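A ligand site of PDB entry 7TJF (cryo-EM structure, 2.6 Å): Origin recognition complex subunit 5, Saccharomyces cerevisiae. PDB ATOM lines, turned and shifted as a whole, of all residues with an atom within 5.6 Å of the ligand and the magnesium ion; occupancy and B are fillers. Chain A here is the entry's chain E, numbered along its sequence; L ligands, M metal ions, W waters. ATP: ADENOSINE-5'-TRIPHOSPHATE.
The side-chain carboxylate (OD2) of Asp 133 lies close to the side-chain hydroxyl (OG1) of Thr 44 (3.2 Å).
The side-chain amino group (NZ) of Lys 43 is in hydrogen-bond range of the side-chain hydroxyl (OG1) of Thr 41 (3.1 Å).
The side-chain amino group (NZ) of Lys 43 sits at hydrogen-bond distance from the backbone carbonyl oxygen (O) of Tyr 38 (2.5 Å).
NZ of Lys 43 lies within hydrogen-bond range of O of Gly 37, at 2.9 Å.
The side-chain hydroxyl (OH) of Tyr 192 sits at hydrogen-bond distance from the backbone carbonyl oxygen (O) of Thr 41 (3.3 Å).
The backbone carbonyl oxygen (O) of Thr 41 is in hydrogen-bond range of the guanidinium group (NH1) of Arg 11 (2.9 Å).
The backbone carbonyl oxygen (O) of Gly 42 lies within hydrogen-bond range of the side-chain hydroxyl (OG1) of Thr 46, 2.8 Å away.
The backbone carbonyl oxygen (O) of Ile 200 lies within hydrogen-bond range of the side-chain hydroxyl (OG) of Ser 204 (3.1 Å).
N of Thr 44 sits at hydrogen-bond distance from O2A of the ligand, 3.5 Å away.
N of Lys 43 lies close to O1B of the ligand, at 3.3 Å.
An oxygen (O1B) of the ligand is in salt-bridge range of the side-chain amino group of Lys 43 (2.7 Å).
N of Tyr 45 sits at hydrogen-bond distance from O2A of the ligand (2.9 Å).
N of Thr 41 is in hydrogen-bond range of O1B of the ligand.
The side-chain hydroxyl (OG1) of Thr 41 lies within hydrogen-bond range of an oxygen (O1B) of the ligand (3.1 Å).
The side-chain hydroxyl of Tyr 192 sits at hydrogen-bond distance from a nitrogen (N7) of the ligand (3.0 Å).
N of Gly 42 lies within hydrogen-bond range of O1B of the ligand (3.1 Å).
O3B of the ligand sits at hydrogen-bond distance from N of Gly 40.
O1B of the ligand sits close to O of Tyr 38.
Residues that only touch the ligand: Val 8 (3.4 Å), Ala 9 (3.99 Å), Ser 39 (3.4 Å), Leu 171 (3.4 Å), Ile 200 (3.6 Å), Met 203 (3.9 Å), Ile 255 (3.9 Å) and Phe 256 (3.7 Å).
Hydrophobic or aromatic side chains within 4 Å of the ligand: Val 8, Tyr 45, Leu 171, Tyr 192, Ile 200, Met 203, Ile 255 and Phe 256.
Of the 22 residues printed, 16 come within 4 Å of the ligand.
Along chain A the residues within 4 Å of the ligand span positions 8 to 256.
The nearest printed residue that does not touch the ligand is Arg 11 (4.2 Å).
One residue has an atom within 4 Å of the magnesium ion: Thr 44.
The nearest printed residue that does not touch the magnesium ion is Asp 133 (4.3 Å).
Water W7 bridges N1 of the ligand and N of Ala 9.
The magnesium ion is bound by water W2 (2.1 Å).
The magnesium ion is bound by water W3 (2.1 Å).
The side-chain hydroxyl (OG1) of Thr 44 binds the magnesium ion.
The magnesium ion is bound by O3G of the ligand (2.2 Å).
The magnesium ion is bound by O2B of the ligand (2.4 Å).
The magnesium ion has five donor atoms within binding distance.
Slightly farther from the magnesium ion lies water W4 (2.8 Å).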
ATOM      1  N   VAL A   8      19.202 -12.234   7.528  1.00  0.00           N
ATOM      2  CA  VAL A   8      18.340 -13.271   8.082  1.00  0.00           C
ATOM      3  C   VAL A   8      18.962 -14.608   7.664  1.00  0.00           C
ATOM      4  O   VAL A   8      19.271 -14.790   6.483  1.00  0.00           O
ATOM      5  CB  VAL A   8      16.882 -13.165   7.592  1.00  0.00           C
ATOM      6  CG1 VAL A   8      15.971 -14.041   8.435  1.00  0.00           C
ATOM      7  CG2 VAL A   8      16.401 -11.719   7.625  1.00  0.00           C
ATOM      8  N   ALA A   9      19.075 -15.531   8.631  1.00  0.00           N
ATOM      9  CA  ALA A   9      20.101 -16.568   8.611  1.00  0.00           C
ATOM     10  C   ALA A   9      19.977 -17.513   7.417  1.00  0.00           C
ATOM     11  O   ALA A   9      20.983 -17.926   6.832  1.00  0.00           O
ATOM     12  CB  ALA A   9      20.058 -17.360   9.912  1.00  0.00           C
ATOM     13  N   PHE A  10      18.755 -17.874   7.039  1.00  0.00           N
ATOM     14  CA  PHE A  10      18.545 -18.744   5.891  1.00  0.00           C
ATOM     15  C   PHE A  10      17.537 -18.135   4.910  1.00  0.00           C
ATOM     16  O   PHE A  10      16.917 -18.867   4.137  1.00  0.00           O
ATOM     17  CB  PHE A  10      18.088 -20.131   6.335  1.00  0.00           C
ATOM     18  CG  PHE A  10      18.976 -20.735   7.386  1.00  0.00           C
ATOM     19  CD1 PHE A  10      20.176 -21.335   7.035  1.00  0.00           C
ATOM     20  CD2 PHE A  10      18.618 -20.698   8.726  1.00  0.00           C
ATOM     21  CE1 PHE A  10      21.001 -21.896   7.993  1.00  0.00           C
ATOM     22  CE2 PHE A  10      19.430 -21.262   9.691  1.00  0.00           C
ATOM     23  CZ  PHE A  10      20.624 -21.854   9.331  1.00  0.00           C
ATOM     24  N   ARG A  11      17.373 -16.819   4.945  1.00  0.00           N
ATOM     25  CA  ARG A  11      16.393 -16.111   4.121  1.00  0.00           C
ATOM     26  C   ARG A  11      17.067 -15.000   3.336  1.00  0.00           C
ATOM     27  O   ARG A  11      16.515 -13.901   3.195  1.00  0.00           O
ATOM     28  CB  ARG A  11      15.255 -15.572   4.980  1.00  0.00           C
ATOM     29  CG  ARG A  11      14.551 -16.585   5.861  1.00  0.00           C
ATOM     30  CD  ARG A  11      13.457 -17.344   5.118  1.00  0.00           C
ATOM     31  NE  ARG A  11      13.965 -18.542   4.455  1.00  0.00           N
ATOM     32  CZ  ARG A  11      13.236 -19.615   4.195  1.00  0.00           C
ATOM     33  NH1 ARG A  11      11.965 -19.690   4.543  1.00  0.00           N
ATOM     34  NH2 ARG A  11      13.794 -20.641   3.569  1.00  0.00           N
ATOM     35  N   GLY A  37       4.151 -18.583   2.092  1.00  0.00           N
ATOM     36  CA  GLY A  37       4.860 -19.630   2.786  1.00  0.00           C
ATOM     37  C   GLY A  37       3.974 -20.263   3.837  1.00  0.00           C
ATOM     38  O   GLY A  37       2.995 -19.666   4.288  1.00  0.00           O
ATOM     39  N   TYR A  38       4.332 -21.479   4.218  1.00  0.00           N
ATOM     40  CA  TYR A  38       3.563 -22.190   5.219  1.00  0.00           C
ATOM     41  C   TYR A  38       3.988 -21.742   6.615  1.00  0.00           C
ATOM     42  O   TYR A  38       4.785 -20.816   6.777  1.00  0.00           O
ATOM     43  CB  TYR A  38       3.692 -23.699   5.027  1.00  0.00           C
ATOM     44  CG  TYR A  38       2.941 -24.167   3.798  1.00  0.00           C
ATOM     45  CD1 TYR A  38       1.595 -24.489   3.878  1.00  0.00           C
ATOM     46  CD2 TYR A  38       3.573 -24.238   2.563  1.00  0.00           C
ATOM     47  CE1 TYR A  38       0.893 -24.905   2.760  1.00  0.00           C
ATOM     48  CE2 TYR A  38       2.873 -24.648   1.438  1.00  0.00           C
ATOM     49  CZ  TYR A  38       1.545 -24.974   1.548  1.00  0.00           C
ATOM     50  OH  TYR A  38       0.856 -25.380   0.431  1.00  0.00           O
ATOM     51  N   SER A  39       3.428 -22.383   7.637  1.00  0.00           N
ATOM     52  CA  SER A  39       3.597 -21.924   9.009  1.00  0.00           C
ATOM     53  C   SER A  39       5.027 -22.118   9.497  1.00  0.00           C
ATOM     54  O   SER A  39       5.643 -23.152   9.260  1.00  0.00           O
ATOM     55  CB  SER A  39       2.628 -22.658   9.936  1.00  0.00           C
ATOM     56  OG  SER A  39       1.344 -22.064   9.892  1.00  0.00           O
ATOM     57  N   GLY A  40       5.542 -21.107  10.183  1.00  0.00           N
ATOM     58  CA  GLY A  40       6.891 -21.148  10.703  1.00  0.00           C
ATOM     59  C   GLY A  40       7.987 -21.054   9.668  1.00  0.00           C
ATOM     60  O   GLY A  40       9.095 -21.513   9.909  1.00  0.00           O
ATOM     61  N   THR A  41       7.700 -20.476   8.506  1.00  0.00           N
ATOM     62  CA  THR A  41       8.701 -20.316   7.466  1.00  0.00           C
ATOM     63  C   THR A  41       9.420 -18.985   7.547  1.00  0.00           C
ATOM     64  O   THR A  41      10.233 -18.673   6.675  1.00  0.00           O
ATOM     65  CB  THR A  41       8.054 -20.492   6.084  1.00  0.00           C
ATOM     66  OG1 THR A  41       6.827 -19.755   6.017  1.00  0.00           O
ATOM     67  CG2 THR A  41       7.782 -21.962   5.814  1.00  0.00           C
ATOM     68  N   GLY A  42       9.135 -18.189   8.572  1.00  0.00           N
ATOM     69  CA  GLY A  42       9.847 -16.944   8.780  1.00  0.00           C
ATOM     70  C   GLY A  42       9.420 -15.782   7.916  1.00  0.00           C
ATOM     71  O   GLY A  42      10.239 -14.906   7.644  1.00  0.00           O
ATOM     72  N   LYS A  43       8.165 -15.760   7.453  1.00  0.00           N
ATOM     73  CA  LYS A  43       7.680 -14.625   6.681  1.00  0.00           C
ATOM     74  C   LYS A  43       7.583 -13.365   7.549  1.00  0.00           C
ATOM     75  O   LYS A  43       8.100 -12.304   7.179  1.00  0.00           O
ATOM     76  CB  LYS A  43       6.313 -14.942   6.062  1.00  0.00           C
ATOM     77  CG  LYS A  43       6.215 -16.299   5.396  1.00  0.00           C
ATOM     78  CD  LYS A  43       4.787 -16.618   4.994  1.00  0.00           C
ATOM     79  CE  LYS A  43       3.913 -17.001   6.188  1.00  0.00           C
ATOM     80  NZ  LYS A  43       4.124 -18.396   6.653  1.00  0.00           N
ATOM     81  N   THR A  44       6.937 -13.495   8.708  1.00  0.00           N
ATOM     82  CA  THR A  44       6.793 -12.372   9.635  1.00  0.00           C
ATOM     83  C   THR A  44       8.145 -11.922  10.171  1.00  0.00           C
ATOM     84  O   THR A  44       8.398 -10.723  10.305  1.00  0.00           O
ATOM     85  CB  THR A  44       5.861 -12.754  10.783  1.00  0.00           C
ATOM     86  OG1 THR A  44       4.657 -13.331  10.260  1.00  0.00           O
ATOM     87  CG2 THR A  44       5.507 -11.547  11.641  1.00  0.00           C
ATOM     88  N   TYR A  45       9.032 -12.880  10.463  1.00  0.00           N
ATOM     89  CA  TYR A  45      10.360 -12.580  10.988  1.00  0.00           C
ATOM     90  C   TYR A  45      11.192 -11.800   9.985  1.00  0.00           C
ATOM     91  O   TYR A  45      11.819 -10.794  10.329  1.00  0.00           O
ATOM     92  CB  TYR A  45      11.058 -13.879  11.390  1.00  0.00           C
ATOM     93  CG  TYR A  45      12.378 -13.691  12.088  1.00  0.00           C
ATOM     94  CD1 TYR A  45      12.418 -13.348  13.440  1.00  0.00           C
ATOM     95  CD2 TYR A  45      13.585 -13.847  11.421  1.00  0.00           C
ATOM     96  CE1 TYR A  45      13.623 -13.172  14.090  1.00  0.00           C
ATOM     97  CE2 TYR A  45      14.784 -13.662  12.062  1.00  0.00           C
ATOM     98  CZ  TYR A  45      14.801 -13.328  13.400  1.00  0.00           C
ATOM     99  OH  TYR A  45      15.997 -13.149  14.049  1.00  0.00           O
ATOM    100  N   THR A  46      11.186 -12.245   8.721  1.00  0.00           N
ATOM    101  CA  THR A  46      11.968 -11.570   7.681  1.00  0.00           C
ATOM    102  C   THR A  46      11.404 -10.188   7.366  1.00  0.00           C
ATOM    103  O   THR A  46      12.165  -9.227   7.211  1.00  0.00           O
ATOM    104  CB  THR A  46      12.013 -12.432   6.413  1.00  0.00           C
ATOM    105  OG1 THR A  46      12.578 -13.710   6.734  1.00  0.00           O
ATOM    106  CG2 THR A  46      12.863 -11.789   5.330  1.00  0.00           C
ATOM    107  N   ASP A 133      -0.825  -9.317   7.018  1.00  0.00           N
ATOM    108  CA  ASP A 133      -0.093 -10.491   7.468  1.00  0.00           C
ATOM    109  C   ASP A 133      -1.052 -11.640   7.776  1.00  0.00           C
ATOM    110  O   ASP A 133      -1.533 -11.756   8.908  1.00  0.00           O
ATOM    111  CB  ASP A 133       0.751 -10.134   8.691  1.00  0.00           C
ATOM    112  CG  ASP A 133       1.871 -11.121   8.971  1.00  0.00           C
ATOM    113  OD1 ASP A 133       1.940 -12.173   8.318  1.00  0.00           O
ATOM    114  OD2 ASP A 133       2.703 -10.827   9.858  1.00  0.00           O
ATOM    115  N   LEU A 171      -0.734 -18.371   3.224  1.00  0.00           N
ATOM    116  CA  LEU A 171      -0.251 -19.684   3.635  1.00  0.00           C
ATOM    117  C   LEU A 171      -0.345 -20.715   2.515  1.00  0.00           C
ATOM    118  O   LEU A 171       0.660 -21.309   2.129  1.00  0.00           O
ATOM    119  CB  LEU A 171      -1.045 -20.171   4.865  1.00  0.00           C
ATOM    120  CG  LEU A 171      -0.631 -19.632   6.238  1.00  0.00           C
ATOM    121  CD1 LEU A 171      -1.701 -19.949   7.273  1.00  0.00           C
ATOM    122  CD2 LEU A 171       0.701 -20.194   6.673  1.00  0.00           C
ATOM    123  N   TYR A 192      11.856 -24.937   6.124  1.00  0.00           N
ATOM    124  CA  TYR A 192      13.231 -25.164   6.541  1.00  0.00           C
ATOM    125  C   TYR A 192      13.531 -26.657   6.607  1.00  0.00           C
ATOM    126  O   TYR A 192      12.634 -27.498   6.694  1.00  0.00           O
ATOM    127  CB  TYR A 192      13.493 -24.541   7.905  1.00  0.00           C
ATOM    128  CG  TYR A 192      13.416 -23.035   7.965  1.00  0.00           C
ATOM    129  CD1 TYR A 192      14.302 -22.239   7.248  1.00  0.00           C
ATOM    130  CD2 TYR A 192      12.459 -22.408   8.756  1.00  0.00           C
ATOM    131  CE1 TYR A 192      14.238 -20.863   7.312  1.00  0.00           C
ATOM    132  CE2 TYR A 192      12.376 -21.026   8.819  1.00  0.00           C
ATOM    133  CZ  TYR A 192      13.270 -20.270   8.099  1.00  0.00           C
ATOM    134  OH  TYR A 192      13.194 -18.897   8.170  1.00  0.00           O
ATOM    135  N   ILE A 200      18.158 -22.393  14.003  1.00  0.00           N
ATOM    136  CA  ILE A 200      17.202 -21.361  14.404  1.00  0.00           C
ATOM    137  C   ILE A 200      16.756 -21.579  15.853  1.00  0.00           C
ATOM    138  O   ILE A 200      16.696 -20.633  16.637  1.00  0.00           O
ATOM    139  CB  ILE A 200      16.013 -21.341  13.427  1.00  0.00           C
ATOM    140  CG1 ILE A 200      16.376 -20.557  12.160  1.00  0.00           C
ATOM    141  CG2 ILE A 200      14.748 -20.769  14.054  1.00  0.00           C
ATOM    142  CD1 ILE A 200      15.421 -20.778  11.011  1.00  0.00           C
ATOM    143  N   MET A 203      19.751 -20.609  18.166  1.00  0.00           N
ATOM    144  CA  MET A 203      19.961 -19.164  18.220  1.00  0.00           C
ATOM    145  C   MET A 203      18.783 -18.420  18.832  1.00  0.00           C
ATOM    146  O   MET A 203      18.965 -17.288  19.302  1.00  0.00           O
ATOM    147  CB  MET A 203      20.286 -18.645  16.817  1.00  0.00           C
ATOM    148  CG  MET A 203      19.171 -17.904  16.096  1.00  0.00           C
ATOM    149  SD  MET A 203      19.660 -17.325  14.463  1.00  0.00           S
ATOM    150  CE  MET A 203      20.095 -18.865  13.667  1.00  0.00           C
ATOM    151  N   SER A 204      17.595 -19.025  18.867  1.00  0.00           N
ATOM    152  CA  SER A 204      16.438 -18.356  19.450  1.00  0.00           C
ATOM    153  C   SER A 204      16.131 -18.776  20.874  1.00  0.00           C
ATOM    154  O   SER A 204      15.432 -18.050  21.580  1.00  0.00           O
ATOM    155  CB  SER A 204      15.198 -18.572  18.581  1.00  0.00           C
ATOM    156  OG  SER A 204      14.615 -19.843  18.838  1.00  0.00           O
ATOM    157  N   ILE A 255       8.783 -25.496  13.718  1.00  0.00           N
ATOM    158  CA  ILE A 255       9.501 -24.748  14.751  1.00  0.00           C
ATOM    159  C   ILE A 255       8.677 -24.673  16.031  1.00  0.00           C
ATOM    160  O   ILE A 255       9.204 -24.826  17.142  1.00  0.00           O
ATOM    161  CB  ILE A 255       9.882 -23.358  14.216  1.00  0.00           C
ATOM    162  CG1 ILE A 255      10.753 -23.475  12.971  1.00  0.00           C
ATOM    163  CG2 ILE A 255      10.582 -22.520  15.290  1.00  0.00           C
ATOM    164  CD1 ILE A 255      11.232 -22.147  12.419  1.00  0.00           C
ATOM    165  N   PHE A 256       7.358 -24.461  15.889  1.00  0.00           N
ATOM    166  CA  PHE A 256       6.492 -24.247  17.055  1.00  0.00           C
ATOM    167  C   PHE A 256       6.355 -25.508  17.899  1.00  0.00           C
ATOM    168  O   PHE A 256       6.458 -25.437  19.130  1.00  0.00           O
ATOM    169  CB  PHE A 256       5.119 -23.756  16.602  1.00  0.00           C
ATOM    170  CG  PHE A 256       5.167 -22.560  15.700  1.00  0.00           C
ATOM    171  CD1 PHE A 256       5.709 -21.357  16.151  1.00  0.00           C
ATOM    172  CD2 PHE A 256       4.673 -22.622  14.410  1.00  0.00           C
ATOM    173  CE1 PHE A 256       5.755 -20.252  15.321  1.00  0.00           C
ATOM    174  CE2 PHE A 256       4.717 -21.525  13.573  1.00  0.00           C
ATOM    175  CZ  PHE A 256       5.262 -20.344  14.033  1.00  0.00           C
HETATM  176  PG  ATP L   1       2.910 -18.218  10.481  1.00  0.00           P
HETATM  177  O1G ATP L   1       2.483 -18.749   9.163  1.00  0.00           O
HETATM  178  O2G ATP L   1       2.536 -19.131  11.651  1.00  0.00           O
HETATM  179  O3G ATP L   1       2.403 -16.814  10.779  1.00  0.00           O
HETATM  180  PB  ATP L   1       5.694 -17.385   9.799  1.00  0.00           P
HETATM  181  O1B ATP L   1       6.008 -18.057   8.525  1.00  0.00           O
HETATM  182  O2B ATP L   1       5.352 -15.903   9.696  1.00  0.00           O
HETATM  183  O3B ATP L   1       4.495 -18.095  10.561  1.00  0.00           O
HETATM  184  PA  ATP L   1       7.521 -16.665  11.991  1.00  0.00           P
HETATM  185  O1A ATP L   1       6.537 -16.325  13.032  1.00  0.00           O
HETATM  186  O2A ATP L   1       8.180 -15.468  11.312  1.00  0.00           O
HETATM  187  O3A ATP L   1       6.880 -17.533  10.845  1.00  0.00           O
HETATM  188  O5' ATP L   1       8.663 -17.604  12.546  1.00  0.00           O
HETATM  189  C5' ATP L   1       8.483 -18.351  13.771  1.00  0.00           C
HETATM  190  C4' ATP L   1       9.597 -18.007  14.727  1.00  0.00           C
HETATM  191  O4' ATP L   1      10.765 -18.774  14.402  1.00  0.00           O
HETATM  192  C3' ATP L   1      10.051 -16.548  14.689  1.00  0.00           C
HETATM  193  O3' ATP L   1       9.253 -15.730  15.530  1.00  0.00           O
HETATM  194  C2' ATP L   1      11.501 -16.646  15.170  1.00  0.00           C
HETATM  195  O2' ATP L   1      11.582 -16.698  16.587  1.00  0.00           O
HETATM  196  C1' ATP L   1      11.929 -17.986  14.563  1.00  0.00           C
HETATM  197  N9  ATP L   1      12.604 -17.866  13.272  1.00  0.00           N
HETATM  198  C8  ATP L   1      12.077 -18.152  12.041  1.00  0.00           C
HETATM  199  N7  ATP L   1      12.906 -17.958  11.052  1.00  0.00           N
HETATM  200  C5  ATP L   1      14.062 -17.508  11.668  1.00  0.00           C
HETATM  201  C6  ATP L   1      15.327 -17.121  11.172  1.00  0.00           C
HETATM  202  N6  ATP L   1      15.646 -17.135   9.878  1.00  0.00           N
HETATM  203  N1  ATP L   1      16.254 -16.722  12.070  1.00  0.00           N
HETATM  204  C2  ATP L   1      15.943 -16.719  13.359  1.00  0.00           C
HETATM  205  N3  ATP L   1      14.790 -17.053  13.949  1.00  0.00           N
HETATM  206  C4  ATP L   1      13.888 -17.446  13.038  1.00  0.00           C
HETATM  207 MG    MG M   1       3.604 -14.972  11.109  1.00  0.00          MG
HETATM  208  O   HOH W   1      15.574 -15.616  16.535  1.00  0.00           O
HETATM  209  O   HOH W   2       4.558 -15.023  12.985  1.00  0.00           O
HETATM  210  O   HOH W   3       2.955 -14.712   9.121  1.00  0.00           O
HETATM  211  O   HOH W   4       0.953 -14.128  11.501  1.00  0.00           O
HETATM  212  O   HOH W   5       0.527 -16.292  12.816  1.00  0.00           O
HETATM  213  O   HOH W   6       8.047 -13.894  14.419  1.00  0.00           O
HETATM  214  O   HOH W   7      18.242 -15.306  11.141  1.00  0.00           O
HETATM  215  O   HOH W   8       0.677 -16.421   8.493  1.00  0.00           O
